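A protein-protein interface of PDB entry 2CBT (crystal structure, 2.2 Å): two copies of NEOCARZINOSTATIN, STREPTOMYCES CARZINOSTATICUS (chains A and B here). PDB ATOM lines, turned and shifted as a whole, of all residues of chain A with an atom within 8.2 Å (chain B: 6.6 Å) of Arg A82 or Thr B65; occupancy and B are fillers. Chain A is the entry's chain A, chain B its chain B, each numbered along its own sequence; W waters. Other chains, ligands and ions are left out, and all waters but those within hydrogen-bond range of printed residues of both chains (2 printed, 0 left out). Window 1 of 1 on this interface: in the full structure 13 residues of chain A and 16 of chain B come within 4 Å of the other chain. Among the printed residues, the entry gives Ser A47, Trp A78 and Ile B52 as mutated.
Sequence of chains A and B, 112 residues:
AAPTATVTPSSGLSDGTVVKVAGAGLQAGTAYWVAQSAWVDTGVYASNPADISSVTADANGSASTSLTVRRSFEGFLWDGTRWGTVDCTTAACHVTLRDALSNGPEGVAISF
OG of Ser B54 is in hydrogen-bond range of O of Gly A80, at 2.5 Å. The side-chain hydroxyl (OG) of Ser B53 is in hydrogen-bond range of the guanidinium group (NH1) of Arg A82, 3.4 Å away. The guanidinium group of Arg A82 sits at hydrogen-bond distance from the backbone carbonyl oxygen of Ser B54, 2.5 Å away. The guanidinium group (NH2) of Arg A82 sits at hydrogen-bond distance from the side-chain hydroxyl (OG1) of Thr B65 (3.5 Å).
N of Ser A47 sits at hydrogen-bond distance from O of Phe A76 (3.0 Å). OG1 of Thr A81 lies close to OD2 of Asp A79, 3.0 Å away. N of Val B34 sits at hydrogen-bond distance from O of Ser B53 (2.5 Å).
Among the printed residues, merely in contact across the chains: Phe A76 with Ser B54 (3.3 Å), Asp A79 with Ala B31 (3.5 Å), Gly A80 with Ala B31 (3.5 Å) and Thr A81 with Ala B31 (3.5 Å).
Of chain B, only Ser B53 (3.4 Å), Ser B54 (2.5 Å) and Thr B65 (3.5 Å) come within 4 Å of Arg A82. Of chain A, only Arg A82 comes within 4 Å of Thr B65. No residue of chain A comes within 4 Å of Ser B64. Of the printed residues of chain B, Thr A81 touches Ala B31. Printed residues of chain A within 4 Å of Ala B31: Asp A79, Gly A80 and Thr A81. Of the printed residues of chain B, Asp A79 touches Ala B31 (3.5 Å). Of the printed residues of chain A, Ser B53 touches Arg A82. Printed residues of chain B within 4 Å of Gly A80: Ala B31 and Ser B54. The nearest residue of chain A that does not touch Thr B65 is Phe A76 (7.9 Å).
Printed residues of chain A that touch a printed residue of chain B: Phe A76, Asp A79, Gly A80, Thr A81 and Arg A82. Hydrophobic or aromatic side chains of chain A that line the printed part of chain B: Phe A76. Hydrophobic or aromatic side chains of chain B that line the printed part of chain A: Ala B31. Among the printed residues, no Asp or Glu carboxylate lies within 4 Å of a Lys or Arg side-chain nitrogen of the other chain.
No position is printed for both chains. Of the 8 pairs that touch across the chains among the printed residues, none has its exchanged pair printed and touching as well.
Water W2 bridges the backbone carbonyl oxygen (O) of Asp A79 (2.8 Å) and the backbone carbonyl oxygen (O) of Ala B31 (3.1 Å). Water W1 bridges the side-chain carboxylate (OD2) of Asp A79 (3.3 Å) and the backbone NH (N) of Ala B31 (3.4 Å).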
ATOM      1  N   ALA A  46       0.850  12.942 -14.622  1.00  0.00           N
ATOM      2  CA  ALA A  46       1.201  14.258 -15.122  1.00  0.00           C
ATOM      3  C   ALA A  46       2.541  14.659 -14.506  1.00  0.00           C
ATOM      4  O   ALA A  46       2.674  14.725 -13.284  1.00  0.00           O
ATOM      5  CB  ALA A  46       0.147  15.305 -14.821  1.00  0.00           C
ATOM      6  N   SER A  47       3.541  14.912 -15.346  1.00  0.00           N
ATOM      7  CA  SER A  47       4.867  15.190 -14.801  1.00  0.00           C
ATOM      8  C   SER A  47       5.381  16.553 -15.229  1.00  0.00           C
ATOM      9  O   SER A  47       4.807  17.216 -16.091  1.00  0.00           O
ATOM     10  CB  SER A  47       5.839  14.091 -15.230  1.00  0.00           C
ATOM     11  OG  SER A  47       5.568  12.857 -14.590  1.00  0.00           O
ATOM     12  N   GLU A  74       3.168  23.096 -14.127  1.00  0.00           N
ATOM     13  CA  GLU A  74       2.215  22.813 -15.215  1.00  0.00           C
ATOM     14  C   GLU A  74       2.427  21.374 -15.682  1.00  0.00           C
ATOM     15  O   GLU A  74       3.550  20.912 -15.908  1.00  0.00           O
ATOM     16  CB  GLU A  74       2.316  23.820 -16.347  1.00  0.00           C
ATOM     17  CG  GLU A  74       3.700  24.107 -16.905  1.00  0.00           C
ATOM     18  CD  GLU A  74       3.649  24.628 -18.325  1.00  0.00           C
ATOM     19  OE1 GLU A  74       3.199  23.876 -19.224  1.00  0.00           O
ATOM     20  OE2 GLU A  74       4.043  25.791 -18.555  1.00  0.00           O
ATOM     21  N   GLY A  75       1.331  20.625 -15.809  1.00  0.00           N
ATOM     22  CA  GLY A  75       1.386  19.202 -16.027  1.00  0.00           C
ATOM     23  C   GLY A  75       1.224  18.738 -17.455  1.00  0.00           C
ATOM     24  O   GLY A  75       0.515  19.322 -18.271  1.00  0.00           O
ATOM     25  N   PHE A  76       1.908  17.640 -17.767  1.00  0.00           N
ATOM     26  CA  PHE A  76       1.838  17.039 -19.087  1.00  0.00           C
ATOM     27  C   PHE A  76       1.651  15.535 -18.925  1.00  0.00           C
ATOM     28  O   PHE A  76       2.217  14.933 -18.016  1.00  0.00           O
ATOM     29  CB  PHE A  76       3.088  17.302 -19.918  1.00  0.00           C
ATOM     30  CG  PHE A  76       3.270  18.702 -20.467  1.00  0.00           C
ATOM     31  CD1 PHE A  76       2.833  19.024 -21.741  1.00  0.00           C
ATOM     32  CD2 PHE A  76       3.880  19.688 -19.716  1.00  0.00           C
ATOM     33  CE1 PHE A  76       2.997  20.297 -22.249  1.00  0.00           C
ATOM     34  CE2 PHE A  76       4.039  20.968 -20.211  1.00  0.00           C
ATOM     35  CZ  PHE A  76       3.596  21.273 -21.482  1.00  0.00           C
ATOM     36  N   LEU A  77       0.858  14.939 -19.808  1.00  0.00           N
ATOM     37  CA  LEU A  77       0.716  13.490 -19.771  1.00  0.00           C
ATOM     38  C   LEU A  77       1.877  12.873 -20.548  1.00  0.00           C
ATOM     39  O   LEU A  77       2.527  13.572 -21.327  1.00  0.00           O
ATOM     40  CB  LEU A  77      -0.606  13.028 -20.369  1.00  0.00           C
ATOM     41  CG  LEU A  77      -1.879  13.737 -19.906  1.00  0.00           C
ATOM     42  CD1 LEU A  77      -3.098  12.873 -20.201  1.00  0.00           C
ATOM     43  CD2 LEU A  77      -1.811  14.094 -18.430  1.00  0.00           C
ATOM     44  N   TRP A  78       2.092  11.583 -20.342  1.00  0.00           N
ATOM     45  CA  TRP A  78       3.146  10.825 -20.995  1.00  0.00           C
ATOM     46  C   TRP A  78       2.851  10.589 -22.474  1.00  0.00           C
ATOM     47  O   TRP A  78       3.596   9.873 -23.149  1.00  0.00           O
ATOM     48  CB  TRP A  78       3.357   9.495 -20.250  1.00  0.00           C
ATOM     49  CG  TRP A  78       3.973   9.693 -18.895  1.00  0.00           C
ATOM     50  CD1 TRP A  78       4.197  10.911 -18.312  1.00  0.00           C
ATOM     51  CD2 TRP A  78       4.440   8.716 -17.957  1.00  0.00           C
ATOM     52  NE1 TRP A  78       4.770  10.745 -17.077  1.00  0.00           N
ATOM     53  CE2 TRP A  78       4.931   9.407 -16.833  1.00  0.00           C
ATOM     54  CE3 TRP A  78       4.505   7.319 -17.935  1.00  0.00           C
ATOM     55  CZ2 TRP A  78       5.470   8.770 -15.716  1.00  0.00           C
ATOM     56  CZ3 TRP A  78       5.036   6.687 -16.828  1.00  0.00           C
ATOM     57  CH2 TRP A  78       5.512   7.407 -15.732  1.00  0.00           C
ATOM     58  N   ASP A  79       1.791  11.178 -23.005  1.00  0.00           N
ATOM     59  CA  ASP A  79       1.422  11.101 -24.413  1.00  0.00           C
ATOM     60  C   ASP A  79       1.580  12.462 -25.084  1.00  0.00           C
ATOM     61  O   ASP A  79       1.496  12.593 -26.304  1.00  0.00           O
ATOM     62  CB  ASP A  79      -0.001  10.563 -24.559  1.00  0.00           C
ATOM     63  CG  ASP A  79      -1.095  11.597 -24.422  1.00  0.00           C
ATOM     64  OD1 ASP A  79      -1.127  12.323 -23.408  1.00  0.00           O
ATOM     65  OD2 ASP A  79      -1.938  11.690 -25.341  1.00  0.00           O
ATOM     66  N   GLY A  80       1.825  13.491 -24.276  1.00  0.00           N
ATOM     67  CA  GLY A  80       2.045  14.835 -24.771  1.00  0.00           C
ATOM     68  C   GLY A  80       1.014  15.837 -24.292  1.00  0.00           C
ATOM     69  O   GLY A  80       1.208  17.049 -24.416  1.00  0.00           O
ATOM     70  N   THR A  81      -0.090  15.341 -23.744  1.00  0.00           N
ATOM     71  CA  THR A  81      -1.204  16.197 -23.344  1.00  0.00           C
ATOM     72  C   THR A  81      -0.853  17.132 -22.193  1.00  0.00           C
ATOM     73  O   THR A  81      -0.405  16.715 -21.128  1.00  0.00           O
ATOM     74  CB  THR A  81      -2.439  15.355 -22.961  1.00  0.00           C
ATOM     75  OG1 THR A  81      -2.461  14.162 -23.754  1.00  0.00           O
ATOM     76  CG2 THR A  81      -3.722  16.115 -23.266  1.00  0.00           C
ATOM     77  N   ARG A  82      -1.076  18.421 -22.435  1.00  0.00           N
ATOM     78  CA  ARG A  82      -0.867  19.483 -21.466  1.00  0.00           C
ATOM     79  C   ARG A  82      -2.085  19.574 -20.539  1.00  0.00           C
ATOM     80  O   ARG A  82      -3.060  20.244 -20.877  1.00  0.00           O
ATOM     81  CB  ARG A  82      -0.620  20.829 -22.143  1.00  0.00           C
ATOM     82  CG  ARG A  82       0.031  21.863 -21.243  1.00  0.00           C
ATOM     83  CD  ARG A  82      -0.267  23.284 -21.692  1.00  0.00           C
ATOM     84  NE  ARG A  82      -0.184  23.448 -23.134  1.00  0.00           N
ATOM     85  CZ  ARG A  82       0.897  23.761 -23.835  1.00  0.00           C
ATOM     86  NH1 ARG A  82       2.067  23.962 -23.246  1.00  0.00           N
ATOM     87  NH2 ARG A  82       0.814  23.877 -25.159  1.00  0.00           N
ATOM     88  N   TRP A  83      -1.965  18.873 -19.425  1.00  0.00           N
ATOM     89  CA  TRP A  83      -2.948  18.760 -18.363  1.00  0.00           C
ATOM     90  C   TRP A  83      -3.053  20.051 -17.555  1.00  0.00           C
ATOM     91  O   TRP A  83      -3.935  20.173 -16.704  1.00  0.00           O
ATOM     92  CB  TRP A  83      -2.568  17.596 -17.456  1.00  0.00           C
ATOM     93  CG  TRP A  83      -3.418  17.371 -16.245  1.00  0.00           C
ATOM     94  CD1 TRP A  83      -3.322  17.965 -15.017  1.00  0.00           C
ATOM     95  CD2 TRP A  83      -4.521  16.457 -16.152  1.00  0.00           C
ATOM     96  NE1 TRP A  83      -4.292  17.484 -14.168  1.00  0.00           N
ATOM     97  CE2 TRP A  83      -5.039  16.557 -14.846  1.00  0.00           C
ATOM     98  CE3 TRP A  83      -5.106  15.565 -17.055  1.00  0.00           C
ATOM     99  CZ2 TRP A  83      -6.128  15.797 -14.420  1.00  0.00           C
ATOM    100  CZ3 TRP A  83      -6.182  14.814 -16.631  1.00  0.00           C
ATOM    101  CH2 TRP A  83      -6.680  14.934 -15.327  1.00  0.00           C
ATOM    102  N   GLY A  84      -2.155  20.996 -17.806  1.00  0.00           N
ATOM    103  CA  GLY A  84      -2.107  22.252 -17.077  1.00  0.00           C
ATOM    104  C   GLY A  84      -1.685  22.064 -15.627  1.00  0.00           C
ATOM    105  O   GLY A  84      -1.350  20.948 -15.222  1.00  0.00           O
ATOM    106  N   THR A  85      -1.700  23.151 -14.875  1.00  0.00           N
ATOM    107  CA  THR A  85      -1.387  23.224 -13.467  1.00  0.00           C
ATOM    108  C   THR A  85      -1.797  21.989 -12.666  1.00  0.00           C
ATOM    109  O   THR A  85      -2.926  21.515 -12.789  1.00  0.00           O
ATOM    110  CB  THR A  85      -2.099  24.417 -12.790  1.00  0.00           C
ATOM    111  OG1 THR A  85      -1.243  25.559 -12.798  1.00  0.00           O
ATOM    112  CG2 THR A  85      -2.382  24.051 -11.343  1.00  0.00           C
ATOM    113  N   VAL B  19       9.377  31.694 -30.300  1.00  0.00           N
ATOM    114  CA  VAL B  19       8.987  31.388 -31.663  1.00  0.00           C
ATOM    115  C   VAL B  19       7.543  30.902 -31.761  1.00  0.00           C
ATOM    116  O   VAL B  19       6.937  30.507 -30.773  1.00  0.00           O
ATOM    117  CB  VAL B  19       9.915  30.315 -32.288  1.00  0.00           C
ATOM    118  CG1 VAL B  19      11.361  30.739 -32.176  1.00  0.00           C
ATOM    119  CG2 VAL B  19       9.678  28.970 -31.613  1.00  0.00           C
ATOM    120  N   LYS B  20       7.016  30.945 -32.984  1.00  0.00           N
ATOM    121  CA  LYS B  20       5.658  30.561 -33.312  1.00  0.00           C
ATOM    122  C   LYS B  20       5.617  29.281 -34.142  1.00  0.00           C
ATOM    123  O   LYS B  20       5.685  29.307 -35.372  1.00  0.00           O
ATOM    124  CB  LYS B  20       4.958  31.679 -34.096  1.00  0.00           C
ATOM    125  CG  LYS B  20       3.509  31.906 -33.684  1.00  0.00           C
ATOM    126  CD  LYS B  20       2.564  31.676 -34.852  1.00  0.00           C
ATOM    127  CE  LYS B  20       3.100  30.606 -35.803  1.00  0.00           C
ATOM    128  NZ  LYS B  20       2.956  31.006 -37.225  1.00  0.00           N
ATOM    129  N   VAL B  21       5.493  28.155 -33.449  1.00  0.00           N
ATOM    130  CA  VAL B  21       5.379  26.876 -34.142  1.00  0.00           C
ATOM    131  C   VAL B  21       3.929  26.597 -34.509  1.00  0.00           C
ATOM    132  O   VAL B  21       3.029  26.829 -33.698  1.00  0.00           O
ATOM    133  CB  VAL B  21       5.925  25.727 -33.276  1.00  0.00           C
ATOM    134  CG1 VAL B  21       6.918  24.891 -34.063  1.00  0.00           C
ATOM    135  CG2 VAL B  21       6.551  26.286 -32.004  1.00  0.00           C
ATOM    136  N   ALA B  22       3.711  26.100 -35.724  1.00  0.00           N
ATOM    137  CA  ALA B  22       2.367  25.778 -36.185  1.00  0.00           C
ATOM    138  C   ALA B  22       2.346  24.430 -36.896  1.00  0.00           C
ATOM    139  O   ALA B  22       3.276  24.099 -37.635  1.00  0.00           O
ATOM    140  CB  ALA B  22       1.832  26.868 -37.100  1.00  0.00           C
ATOM    141  N   ALA B  31      -1.834  14.691 -29.352  1.00  0.00           N
ATOM    142  CA  ALA B  31      -0.889  15.475 -28.584  1.00  0.00           C
ATOM    143  C   ALA B  31       0.516  15.417 -29.174  1.00  0.00           C
ATOM    144  O   ALA B  31       1.096  14.356 -29.403  1.00  0.00           O
ATOM    145  CB  ALA B  31      -0.854  14.991 -27.140  1.00  0.00           C
ATOM    146  N   VAL B  34       6.432  19.667 -28.070  1.00  0.00           N
ATOM    147  CA  VAL B  34       7.070  20.731 -28.845  1.00  0.00           C
ATOM    148  C   VAL B  34       8.442  21.033 -28.260  1.00  0.00           C
ATOM    149  O   VAL B  34       8.572  21.613 -27.186  1.00  0.00           O
ATOM    150  CB  VAL B  34       6.208  22.005 -28.880  1.00  0.00           C
ATOM    151  CG1 VAL B  34       7.016  23.197 -29.363  1.00  0.00           C
ATOM    152  CG2 VAL B  34       4.987  21.791 -29.766  1.00  0.00           C
ATOM    153  N   ILE B  52      10.230  22.940 -23.137  1.00  0.00           N
ATOM    154  CA  ILE B  52       9.305  22.149 -23.937  1.00  0.00           C
ATOM    155  C   ILE B  52       7.897  22.740 -23.998  1.00  0.00           C
ATOM    156  O   ILE B  52       7.420  23.486 -23.153  1.00  0.00           O
ATOM    157  CB  ILE B  52       9.188  20.709 -23.398  1.00  0.00           C
ATOM    158  CG1 ILE B  52       9.237  19.628 -24.476  1.00  0.00           C
ATOM    159  CG2 ILE B  52       7.929  20.560 -22.554  1.00  0.00           C
ATOM    160  CD1 ILE B  52       8.951  18.235 -23.963  1.00  0.00           C
ATOM    161  N   SER B  53       7.188  22.373 -25.064  1.00  0.00           N
ATOM    162  CA  SER B  53       5.778  22.721 -25.167  1.00  0.00           C
ATOM    163  C   SER B  53       5.021  21.515 -25.719  1.00  0.00           C
ATOM    164  O   SER B  53       5.594  20.438 -25.849  1.00  0.00           O
ATOM    165  CB  SER B  53       5.543  23.948 -26.043  1.00  0.00           C
ATOM    166  OG  SER B  53       4.309  24.569 -25.724  1.00  0.00           O
ATOM    167  N   SER B  54       3.749  21.728 -26.032  1.00  0.00           N
ATOM    168  CA  SER B  54       2.912  20.658 -26.570  1.00  0.00           C
ATOM    169  C   SER B  54       1.719  21.256 -27.291  1.00  0.00           C
ATOM    170  O   SER B  54       1.331  22.402 -27.059  1.00  0.00           O
ATOM    171  CB  SER B  54       2.478  19.715 -25.452  1.00  0.00           C
ATOM    172  OG  SER B  54       1.145  19.276 -25.610  1.00  0.00           O
ATOM    173  N   VAL B  55       1.113  20.491 -28.198  1.00  0.00           N
ATOM    174  CA  VAL B  55      -0.025  21.068 -28.917  1.00  0.00           C
ATOM    175  C   VAL B  55      -1.026  19.977 -29.273  1.00  0.00           C
ATOM    176  O   VAL B  55      -0.682  18.952 -29.861  1.00  0.00           O
ATOM    177  CB  VAL B  55       0.424  21.831 -30.175  1.00  0.00           C
ATOM    178  CG1 VAL B  55      -0.033  21.154 -31.451  1.00  0.00           C
ATOM    179  CG2 VAL B  55      -0.104  23.263 -30.114  1.00  0.00           C
ATOM    180  N   THR B  56      -2.278  20.223 -28.889  1.00  0.00           N
ATOM    181  CA  THR B  56      -3.346  19.272 -29.178  1.00  0.00           C
ATOM    182  C   THR B  56      -4.056  19.676 -30.462  1.00  0.00           C
ATOM    183  O   THR B  56      -4.672  20.734 -30.563  1.00  0.00           O
ATOM    184  CB  THR B  56      -4.336  19.170 -28.007  1.00  0.00           C
ATOM    185  OG1 THR B  56      -3.613  18.769 -26.833  1.00  0.00           O
ATOM    186  CG2 THR B  56      -5.368  18.090 -28.270  1.00  0.00           C
ATOM    187  N   ALA B  63      -3.178  23.454 -34.881  1.00  0.00           N
ATOM    188  CA  ALA B  63      -3.033  24.032 -33.555  1.00  0.00           C
ATOM    189  C   ALA B  63      -1.663  24.689 -33.431  1.00  0.00           C
ATOM    190  O   ALA B  63      -0.778  24.445 -34.253  1.00  0.00           O
ATOM    191  CB  ALA B  63      -3.221  23.010 -32.443  1.00  0.00           C
ATOM    192  N   SER B  64      -1.465  25.519 -32.409  1.00  0.00           N
ATOM    193  CA  SER B  64      -0.190  26.227 -32.302  1.00  0.00           C
ATOM    194  C   SER B  64       0.126  26.602 -30.865  1.00  0.00           C
ATOM    195  O   SER B  64      -0.737  26.526 -29.988  1.00  0.00           O
ATOM    196  CB  SER B  64      -0.221  27.481 -33.178  1.00  0.00           C
ATOM    197  OG  SER B  64      -1.110  28.464 -32.686  1.00  0.00           O
ATOM    198  N   THR B  65       1.363  27.019 -30.591  1.00  0.00           N
ATOM    199  CA  THR B  65       1.686  27.443 -29.228  1.00  0.00           C
ATOM    200  C   THR B  65       3.009  28.202 -29.221  1.00  0.00           C
ATOM    201  O   THR B  65       3.656  28.330 -30.262  1.00  0.00           O
ATOM    202  CB  THR B  65       1.751  26.265 -28.241  1.00  0.00           C
ATOM    203  OG1 THR B  65       1.647  26.747 -26.890  1.00  0.00           O
ATOM    204  CG2 THR B  65       3.083  25.539 -28.340  1.00  0.00           C
ATOM    205  N   SER B  66       3.382  28.695 -28.043  1.00  0.00           N
ATOM    206  CA  SER B  66       4.596  29.473 -27.868  1.00  0.00           C
ATOM    207  C   SER B  66       5.777  28.631 -27.395  1.00  0.00           C
ATOM    208  O   SER B  66       5.709  27.869 -26.434  1.00  0.00           O
ATOM    209  CB  SER B  66       4.349  30.607 -26.866  1.00  0.00           C
ATOM    210  OG  SER B  66       5.448  30.716 -25.934  1.00  0.00           O
ATOM    211  N   LEU B  67       6.894  28.798 -28.100  1.00  0.00           N
ATOM    212  CA  LEU B  67       8.144  28.156 -27.721  1.00  0.00           C
ATOM    213  C   LEU B  67       9.219  29.213 -27.501  1.00  0.00           C
ATOM    214  O   LEU B  67       9.273  30.202 -28.232  1.00  0.00           O
ATOM    215  CB  LEU B  67       8.582  27.160 -28.792  1.00  0.00           C
ATOM    216  CG  LEU B  67       9.798  26.302 -28.441  1.00  0.00           C
ATOM    217  CD1 LEU B  67       9.871  26.031 -26.947  1.00  0.00           C
ATOM    218  CD2 LEU B  67       9.778  25.000 -29.226  1.00  0.00           C
HETATM  219  O   HOH W   1      -3.719  12.128 -28.044  1.00  0.00           O
HETATM  220  O   HOH W   2       0.364  11.421 -28.635  1.00  0.00           O
